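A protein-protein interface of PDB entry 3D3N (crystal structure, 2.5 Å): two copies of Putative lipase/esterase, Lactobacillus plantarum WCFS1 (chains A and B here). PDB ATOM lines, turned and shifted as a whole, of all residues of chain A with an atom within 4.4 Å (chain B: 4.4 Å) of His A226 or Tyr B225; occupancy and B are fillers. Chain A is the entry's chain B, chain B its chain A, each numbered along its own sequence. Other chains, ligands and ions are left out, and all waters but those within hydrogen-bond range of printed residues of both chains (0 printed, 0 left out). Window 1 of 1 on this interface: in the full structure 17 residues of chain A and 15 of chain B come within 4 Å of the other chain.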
ATOM      1  N   PHE A 194      10.009 -17.701 -24.405  1.00  0.00           N
ATOM      2  CA  PHE A 194      10.195 -18.376 -23.132  1.00  0.00           C
ATOM      3  C   PHE A 194      10.325 -17.266 -22.098  1.00  0.00           C
ATOM      4  O   PHE A 194      11.258 -16.481 -22.160  1.00  0.00           O
ATOM      5  CB  PHE A 194      11.464 -19.223 -23.176  1.00  0.00           C
ATOM      6  CG  PHE A 194      11.749 -19.934 -21.898  1.00  0.00           C
ATOM      7  CD1 PHE A 194      12.361 -19.272 -20.841  1.00  0.00           C
ATOM      8  CD2 PHE A 194      11.379 -21.266 -21.737  1.00  0.00           C
ATOM      9  CE1 PHE A 194      12.601 -19.925 -19.636  1.00  0.00           C
ATOM     10  CE2 PHE A 194      11.611 -21.932 -20.537  1.00  0.00           C
ATOM     11  CZ  PHE A 194      12.226 -21.260 -19.482  1.00  0.00           C
ATOM     12  N   VAL A 195       9.396 -17.204 -21.153  1.00  0.00           N
ATOM     13  CA  VAL A 195       9.409 -16.142 -20.153  1.00  0.00           C
ATOM     14  C   VAL A 195       9.611 -16.628 -18.722  1.00  0.00           C
ATOM     15  O   VAL A 195       9.058 -17.646 -18.316  1.00  0.00           O
ATOM     16  CB  VAL A 195       8.092 -15.348 -20.218  1.00  0.00           C
ATOM     17  CG1 VAL A 195       8.177 -14.118 -19.340  1.00  0.00           C
ATOM     18  CG2 VAL A 195       7.803 -14.964 -21.651  1.00  0.00           C
ATOM     19  N   TRP A 196      10.403 -15.895 -17.955  1.00  0.00           N
ATOM     20  CA  TRP A 196      10.650 -16.280 -16.577  1.00  0.00           C
ATOM     21  C   TRP A 196      10.918 -15.041 -15.731  1.00  0.00           C
ATOM     22  O   TRP A 196      11.339 -14.002 -16.247  1.00  0.00           O
ATOM     23  CB  TRP A 196      11.845 -17.244 -16.479  1.00  0.00           C
ATOM     24  CG  TRP A 196      13.182 -16.582 -16.641  1.00  0.00           C
ATOM     25  CD1 TRP A 196      13.813 -16.284 -17.811  1.00  0.00           C
ATOM     26  CD2 TRP A 196      14.010 -16.061 -15.592  1.00  0.00           C
ATOM     27  NE1 TRP A 196      14.979 -15.607 -17.557  1.00  0.00           N
ATOM     28  CE2 TRP A 196      15.125 -15.456 -16.202  1.00  0.00           C
ATOM     29  CE3 TRP A 196      13.914 -16.048 -14.191  1.00  0.00           C
ATOM     30  CZ2 TRP A 196      16.144 -14.839 -15.463  1.00  0.00           C
ATOM     31  CZ3 TRP A 196      14.926 -15.434 -13.456  1.00  0.00           C
ATOM     32  CH2 TRP A 196      16.024 -14.839 -14.095  1.00  0.00           C
ATOM     33  N   GLN A 197      10.682 -15.175 -14.429  1.00  0.00           N
ATOM     34  CA  GLN A 197      10.863 -14.090 -13.480  1.00  0.00           C
ATOM     35  C   GLN A 197      10.470 -14.563 -12.084  1.00  0.00           C
ATOM     36  O   GLN A 197       9.713 -15.527 -11.943  1.00  0.00           O
ATOM     37  CB  GLN A 197       9.976 -12.905 -13.877  1.00  0.00           C
ATOM     38  CG  GLN A 197       9.871 -11.814 -12.818  1.00  0.00           C
ATOM     39  CD  GLN A 197       9.003 -10.648 -13.254  1.00  0.00           C
ATOM     40  OE1 GLN A 197       7.855 -10.835 -13.637  1.00  0.00           O
ATOM     41  NE2 GLN A 197       9.551  -9.433 -13.189  1.00  0.00           N
ATOM     42  N   TYR A 225       5.999 -20.100 -19.497  1.00  0.00           N
ATOM     43  CA  TYR A 225       6.165 -19.105 -18.449  1.00  0.00           C
ATOM     44  C   TYR A 225       6.504 -19.748 -17.120  1.00  0.00           C
ATOM     45  O   TYR A 225       5.866 -20.711 -16.708  1.00  0.00           O
ATOM     46  CB  TYR A 225       4.895 -18.267 -18.317  1.00  0.00           C
ATOM     47  CG  TYR A 225       4.954 -17.228 -17.225  1.00  0.00           C
ATOM     48  CD1 TYR A 225       6.062 -16.399 -17.072  1.00  0.00           C
ATOM     49  CD2 TYR A 225       3.888 -17.057 -16.354  1.00  0.00           C
ATOM     50  CE1 TYR A 225       6.099 -15.424 -16.077  1.00  0.00           C
ATOM     51  CE2 TYR A 225       3.916 -16.089 -15.360  1.00  0.00           C
ATOM     52  CZ  TYR A 225       5.021 -15.278 -15.228  1.00  0.00           C
ATOM     53  OH  TYR A 225       5.012 -14.320 -14.248  1.00  0.00           O
ATOM     54  N   HIS A 226       7.516 -19.207 -16.455  1.00  0.00           N
ATOM     55  CA  HIS A 226       7.955 -19.734 -15.176  1.00  0.00           C
ATOM     56  C   HIS A 226       8.210 -18.632 -14.160  1.00  0.00           C
ATOM     57  O   HIS A 226       9.263 -18.002 -14.160  1.00  0.00           O
ATOM     58  CB  HIS A 226       9.228 -20.552 -15.368  1.00  0.00           C
ATOM     59  CG  HIS A 226       9.053 -21.726 -16.273  1.00  0.00           C
ATOM     60  ND1 HIS A 226       8.248 -22.798 -15.954  1.00  0.00           N
ATOM     61  CD2 HIS A 226       9.561 -21.990 -17.501  1.00  0.00           C
ATOM     62  CE1 HIS A 226       8.267 -23.671 -16.945  1.00  0.00           C
ATOM     63  NE2 HIS A 226       9.055 -23.205 -17.896  1.00  0.00           N
ATOM     64  N   LEU A 227       7.229 -18.408 -13.299  1.00  0.00           N
ATOM     65  CA  LEU A 227       7.330 -17.408 -12.257  1.00  0.00           C
ATOM     66  C   LEU A 227       7.710 -18.152 -10.979  1.00  0.00           C
ATOM     67  O   LEU A 227       6.866 -18.782 -10.339  1.00  0.00           O
ATOM     68  CB  LEU A 227       5.984 -16.710 -12.090  1.00  0.00           C
ATOM     69  CG  LEU A 227       5.855 -15.601 -11.045  1.00  0.00           C
ATOM     70  CD1 LEU A 227       6.642 -14.381 -11.478  1.00  0.00           C
ATOM     71  CD2 LEU A 227       4.379 -15.243 -10.888  1.00  0.00           C
ATOM     72  N   PHE A 228       8.990 -18.098 -10.632  1.00  0.00           N
ATOM     73  CA  PHE A 228       9.510 -18.759  -9.445  1.00  0.00           C
ATOM     74  C   PHE A 228       9.114 -18.007  -8.189  1.00  0.00           C
ATOM     75  O   PHE A 228       9.151 -16.781  -8.158  1.00  0.00           O
ATOM     76  CB  PHE A 228      11.034 -18.841  -9.535  1.00  0.00           C
ATOM     77  CG  PHE A 228      11.520 -19.697 -10.660  1.00  0.00           C
ATOM     78  CD1 PHE A 228      11.650 -21.070 -10.496  1.00  0.00           C
ATOM     79  CD2 PHE A 228      11.800 -19.143 -11.902  1.00  0.00           C
ATOM     80  CE1 PHE A 228      12.053 -21.880 -11.553  1.00  0.00           C
ATOM     81  CE2 PHE A 228      12.201 -19.946 -12.965  1.00  0.00           C
ATOM     82  CZ  PHE A 228      12.327 -21.317 -12.788  1.00  0.00           C
ATOM     83  N   LEU A 261      15.551 -24.994 -17.916  1.00  0.00           N
ATOM     84  CA  LEU A 261      14.221 -25.022 -18.497  1.00  0.00           C
ATOM     85  C   LEU A 261      14.268 -24.425 -19.897  1.00  0.00           C
ATOM     86  O   LEU A 261      13.880 -25.074 -20.861  1.00  0.00           O
ATOM     87  CB  LEU A 261      13.242 -24.234 -17.627  1.00  0.00           C
ATOM     88  CG  LEU A 261      13.172 -24.653 -16.158  1.00  0.00           C
ATOM     89  CD1 LEU A 261      12.212 -23.731 -15.430  1.00  0.00           C
ATOM     90  CD2 LEU A 261      12.730 -26.101 -16.039  1.00  0.00           C
ATOM     91  N   VAL B 195       1.267 -23.157  -8.523  1.00  0.00           N
ATOM     92  CA  VAL B 195       0.424 -23.470  -9.667  1.00  0.00           C
ATOM     93  C   VAL B 195       1.220 -23.863 -10.909  1.00  0.00           C
ATOM     94  O   VAL B 195       2.254 -23.277 -11.204  1.00  0.00           O
ATOM     95  CB  VAL B 195      -0.478 -22.251 -10.009  1.00  0.00           C
ATOM     96  CG1 VAL B 195      -1.408 -22.586 -11.150  1.00  0.00           C
ATOM     97  CG2 VAL B 195      -1.273 -21.831  -8.782  1.00  0.00           C
ATOM     98  N   GLN B 197       0.804 -25.775 -15.123  1.00  0.00           N
ATOM     99  CA  GLN B 197      -0.067 -26.268 -16.190  1.00  0.00           C
ATOM    100  C   GLN B 197       0.649 -26.210 -17.537  1.00  0.00           C
ATOM    101  O   GLN B 197       1.627 -25.479 -17.692  1.00  0.00           O
ATOM    102  CB  GLN B 197      -1.338 -25.414 -16.255  1.00  0.00           C
ATOM    103  CG  GLN B 197      -2.253 -25.738 -17.432  1.00  0.00           C
ATOM    104  CD  GLN B 197      -3.480 -24.838 -17.490  1.00  0.00           C
ATOM    105  OE1 GLN B 197      -3.364 -23.617 -17.428  1.00  0.00           O
ATOM    106  NE2 GLN B 197      -4.661 -25.440 -17.620  1.00  0.00           N
ATOM    107  N   PRO B 206      -5.820 -22.278 -20.191  1.00  0.00           N
ATOM    108  CA  PRO B 206      -4.701 -21.766 -19.392  1.00  0.00           C
ATOM    109  C   PRO B 206      -4.967 -20.423 -18.730  1.00  0.00           C
ATOM    110  O   PRO B 206      -4.330 -20.083 -17.736  1.00  0.00           O
ATOM    111  CB  PRO B 206      -3.566 -21.681 -20.405  1.00  0.00           C
ATOM    112  CG  PRO B 206      -3.867 -22.797 -21.326  1.00  0.00           C
ATOM    113  CD  PRO B 206      -5.350 -22.635 -21.540  1.00  0.00           C
ATOM    114  N   SER B 209      -5.559 -20.336 -14.926  1.00  0.00           N
ATOM    115  CA  SER B 209      -4.389 -20.278 -14.061  1.00  0.00           C
ATOM    116  C   SER B 209      -3.941 -18.834 -13.893  1.00  0.00           C
ATOM    117  O   SER B 209      -3.803 -18.339 -12.775  1.00  0.00           O
ATOM    118  CB  SER B 209      -3.255 -21.079 -14.680  1.00  0.00           C
ATOM    119  OG  SER B 209      -3.760 -22.243 -15.288  1.00  0.00           O
ATOM    120  N   LEU B 210      -3.708 -18.170 -15.020  1.00  0.00           N
ATOM    121  CA  LEU B 210      -3.272 -16.775 -15.023  1.00  0.00           C
ATOM    122  C   LEU B 210      -4.135 -15.928 -14.109  1.00  0.00           C
ATOM    123  O   LEU B 210      -3.626 -15.228 -13.233  1.00  0.00           O
ATOM    124  CB  LEU B 210      -3.327 -16.198 -16.439  1.00  0.00           C
ATOM    125  CG  LEU B 210      -2.235 -16.647 -17.416  1.00  0.00           C
ATOM    126  CD1 LEU B 210      -2.578 -16.189 -18.833  1.00  0.00           C
ATOM    127  CD2 LEU B 210      -0.901 -16.073 -16.983  1.00  0.00           C
ATOM    128  N   VAL B 213      -3.353 -16.747 -10.449  1.00  0.00           N
ATOM    129  CA  VAL B 213      -2.012 -16.328 -10.071  1.00  0.00           C
ATOM    130  C   VAL B 213      -1.882 -14.809  -9.923  1.00  0.00           C
ATOM    131  O   VAL B 213      -1.143 -14.323  -9.065  1.00  0.00           O
ATOM    132  CB  VAL B 213      -0.981 -16.826 -11.093  1.00  0.00           C
ATOM    133  CG1 VAL B 213       0.394 -16.268 -10.766  1.00  0.00           C
ATOM    134  CG2 VAL B 213      -0.956 -18.346 -11.082  1.00  0.00           C
ATOM    135  N   ALA B 224       3.912 -19.378  -6.941  1.00  0.00           N
ATOM    136  CA  ALA B 224       4.825 -19.944  -7.921  1.00  0.00           C
ATOM    137  C   ALA B 224       3.987 -20.465  -9.088  1.00  0.00           C
ATOM    138  O   ALA B 224       3.148 -21.344  -8.916  1.00  0.00           O
ATOM    139  CB  ALA B 224       5.626 -21.069  -7.290  1.00  0.00           C
ATOM    140  N   TYR B 225       4.205 -19.907 -10.272  1.00  0.00           N
ATOM    141  CA  TYR B 225       3.454 -20.314 -11.453  1.00  0.00           C
ATOM    142  C   TYR B 225       4.378 -20.909 -12.508  1.00  0.00           C
ATOM    143  O   TYR B 225       5.409 -20.336 -12.839  1.00  0.00           O
ATOM    144  CB  TYR B 225       2.702 -19.105 -12.015  1.00  0.00           C
ATOM    145  CG  TYR B 225       1.781 -19.424 -13.165  1.00  0.00           C
ATOM    146  CD1 TYR B 225       1.058 -20.612 -13.199  1.00  0.00           C
ATOM    147  CD2 TYR B 225       1.591 -18.512 -14.203  1.00  0.00           C
ATOM    148  CE1 TYR B 225       0.171 -20.883 -14.233  1.00  0.00           C
ATOM    149  CE2 TYR B 225       0.704 -18.773 -15.242  1.00  0.00           C
ATOM    150  CZ  TYR B 225      -0.003 -19.961 -15.244  1.00  0.00           C
ATOM    151  OH  TYR B 225      -0.905 -20.218 -16.245  1.00  0.00           O
ATOM    152  N   HIS B 226       4.010 -22.065 -13.040  1.00  0.00           N
ATOM    153  CA  HIS B 226       4.834 -22.707 -14.046  1.00  0.00           C
ATOM    154  C   HIS B 226       4.002 -23.205 -15.215  1.00  0.00           C
ATOM    155  O   HIS B 226       3.385 -24.272 -15.165  1.00  0.00           O
ATOM    156  CB  HIS B 226       5.598 -23.867 -13.421  1.00  0.00           C
ATOM    157  CG  HIS B 226       6.601 -23.441 -12.402  1.00  0.00           C
ATOM    158  ND1 HIS B 226       7.738 -22.731 -12.728  1.00  0.00           N
ATOM    159  CD2 HIS B 226       6.631 -23.601 -11.059  1.00  0.00           C
ATOM    160  CE1 HIS B 226       8.424 -22.472 -11.631  1.00  0.00           C
ATOM    161  NE2 HIS B 226       7.773 -22.988 -10.603  1.00  0.00           N
ATOM    162  N   LEU B 227       3.980 -22.417 -16.275  1.00  0.00           N
ATOM    163  CA  LEU B 227       3.237 -22.792 -17.454  1.00  0.00           C
ATOM    164  C   LEU B 227       4.216 -23.394 -18.462  1.00  0.00           C
ATOM    165  O   LEU B 227       4.865 -22.683 -19.231  1.00  0.00           O
ATOM    166  CB  LEU B 227       2.536 -21.561 -18.020  1.00  0.00           C
ATOM    167  CG  LEU B 227       1.865 -21.663 -19.382  1.00  0.00           C
ATOM    168  CD1 LEU B 227       0.906 -22.836 -19.423  1.00  0.00           C
ATOM    169  CD2 LEU B 227       1.139 -20.353 -19.662  1.00  0.00           C
ATOM    170  N   PHE B 228       4.332 -24.714 -18.430  1.00  0.00           N
ATOM    171  CA  PHE B 228       5.226 -25.424 -19.321  1.00  0.00           C
ATOM    172  C   PHE B 228       4.788 -25.284 -20.770  1.00  0.00           C
ATOM    173  O   PHE B 228       3.595 -25.187 -21.060  1.00  0.00           O
ATOM    174  CB  PHE B 228       5.275 -26.895 -18.913  1.00  0.00           C
ATOM    175  CG  PHE B 228       5.798 -27.113 -17.525  1.00  0.00           C
ATOM    176  CD1 PHE B 228       7.148 -26.962 -17.250  1.00  0.00           C
ATOM    177  CD2 PHE B 228       4.937 -27.434 -16.483  1.00  0.00           C
ATOM    178  CE1 PHE B 228       7.640 -27.126 -15.953  1.00  0.00           C
ATOM    179  CE2 PHE B 228       5.419 -27.600 -15.183  1.00  0.00           C
ATOM    180  CZ  PHE B 228       6.774 -27.445 -14.921  1.00  0.00           C
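The backbone carbonyl oxygen (O) of Tyr B225 lies within hydrogen-bond range of the backbone NH (N) of Leu A227, 2.7 Å away.
ND1 of His B226 is in hydrogen-bond range of ND1 of His A226 (3.3 Å).
O of Tyr A225 is in hydrogen-bond range of N of Leu B227 (2.6 Å).
O of Ala B224 is in hydrogen-bond range of N of Val B195.
The backbone carbonyl oxygen (O) of Val B195 lies within hydrogen-bond range of the backbone NH (N) of His B226 (2.8 Å).
The backbone NH of Gln B197 lies within hydrogen-bond range of the backbone carbonyl oxygen of His B226 (3.0 Å).
O of Gln B197 lies within hydrogen-bond range of N of Phe B228 (2.9 Å).
The backbone NH (N) of His A226 lies within hydrogen-bond range of the backbone carbonyl oxygen (O) of Val A195 (2.9 Å).
O of His A226 is in hydrogen-bond range of N of Gln A197 (3.2 Å).
Tyr A225 touches Tyr B225.
C of His B226 touches O of Tyr A225, at 3.5 Å.
His A226 touches Tyr B225 (CA to O, 3.5 Å).
His A226 touches Phe B228 (CE1 to CD1, 3.5 Å).
Leu A227 touches Ala B224 (O to CA, 3.4 Å).
Phe A228 touches His B226 (CE1 to CE1, 3.7 Å).
Of chain B, only Tyr B225, His B226 and Phe B228 come within 4 Å of His A226.
Of the printed residues of chain B, Phe A228 touches His B226.
Ser B209 touches none of the printed residues of chain A.
Printed residues of chain A within 4 Å of Ala B224: Leu A227.
Tyr B225 touches just these residues of chain A: Tyr A225, His A226 and Leu A227.
Printed residues of chain A within 4 Å of His B226: Tyr A225, His A226 and Phe A228.
Of the printed residues of chain A, Leu B227 touches Tyr A225 (2.6 Å).
Of the printed residues of chain A, Phe B228 touches His A226.
The nearest residue of chain B that does not touch His A226 is Leu B227 (4.2 Å).
The nearest printed residue of chain A that does not touch Ala B224 is Phe A228 (4.7 Å).
Hydrophobic or aromatic side chains of chain A that line the printed part of chain B: Tyr A225, His A226, Leu A227 and Phe A228.
Among the printed residues, 9 pairs touch across the chains.
Tyr A225 touches its own counterpart, Tyr B225.
Tyr A225 touches Leu B227, and with the chains exchanged Leu A227 touches Tyr B225.
His B226 touches its own counterpart, His A226.
His A226 touches Phe B228, and with the chains exchanged Phe A228 touches His B226.
Of the 9 pairs that touch across the chains among the printed residues, 8 have their exchanged pair printed and touching as well.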
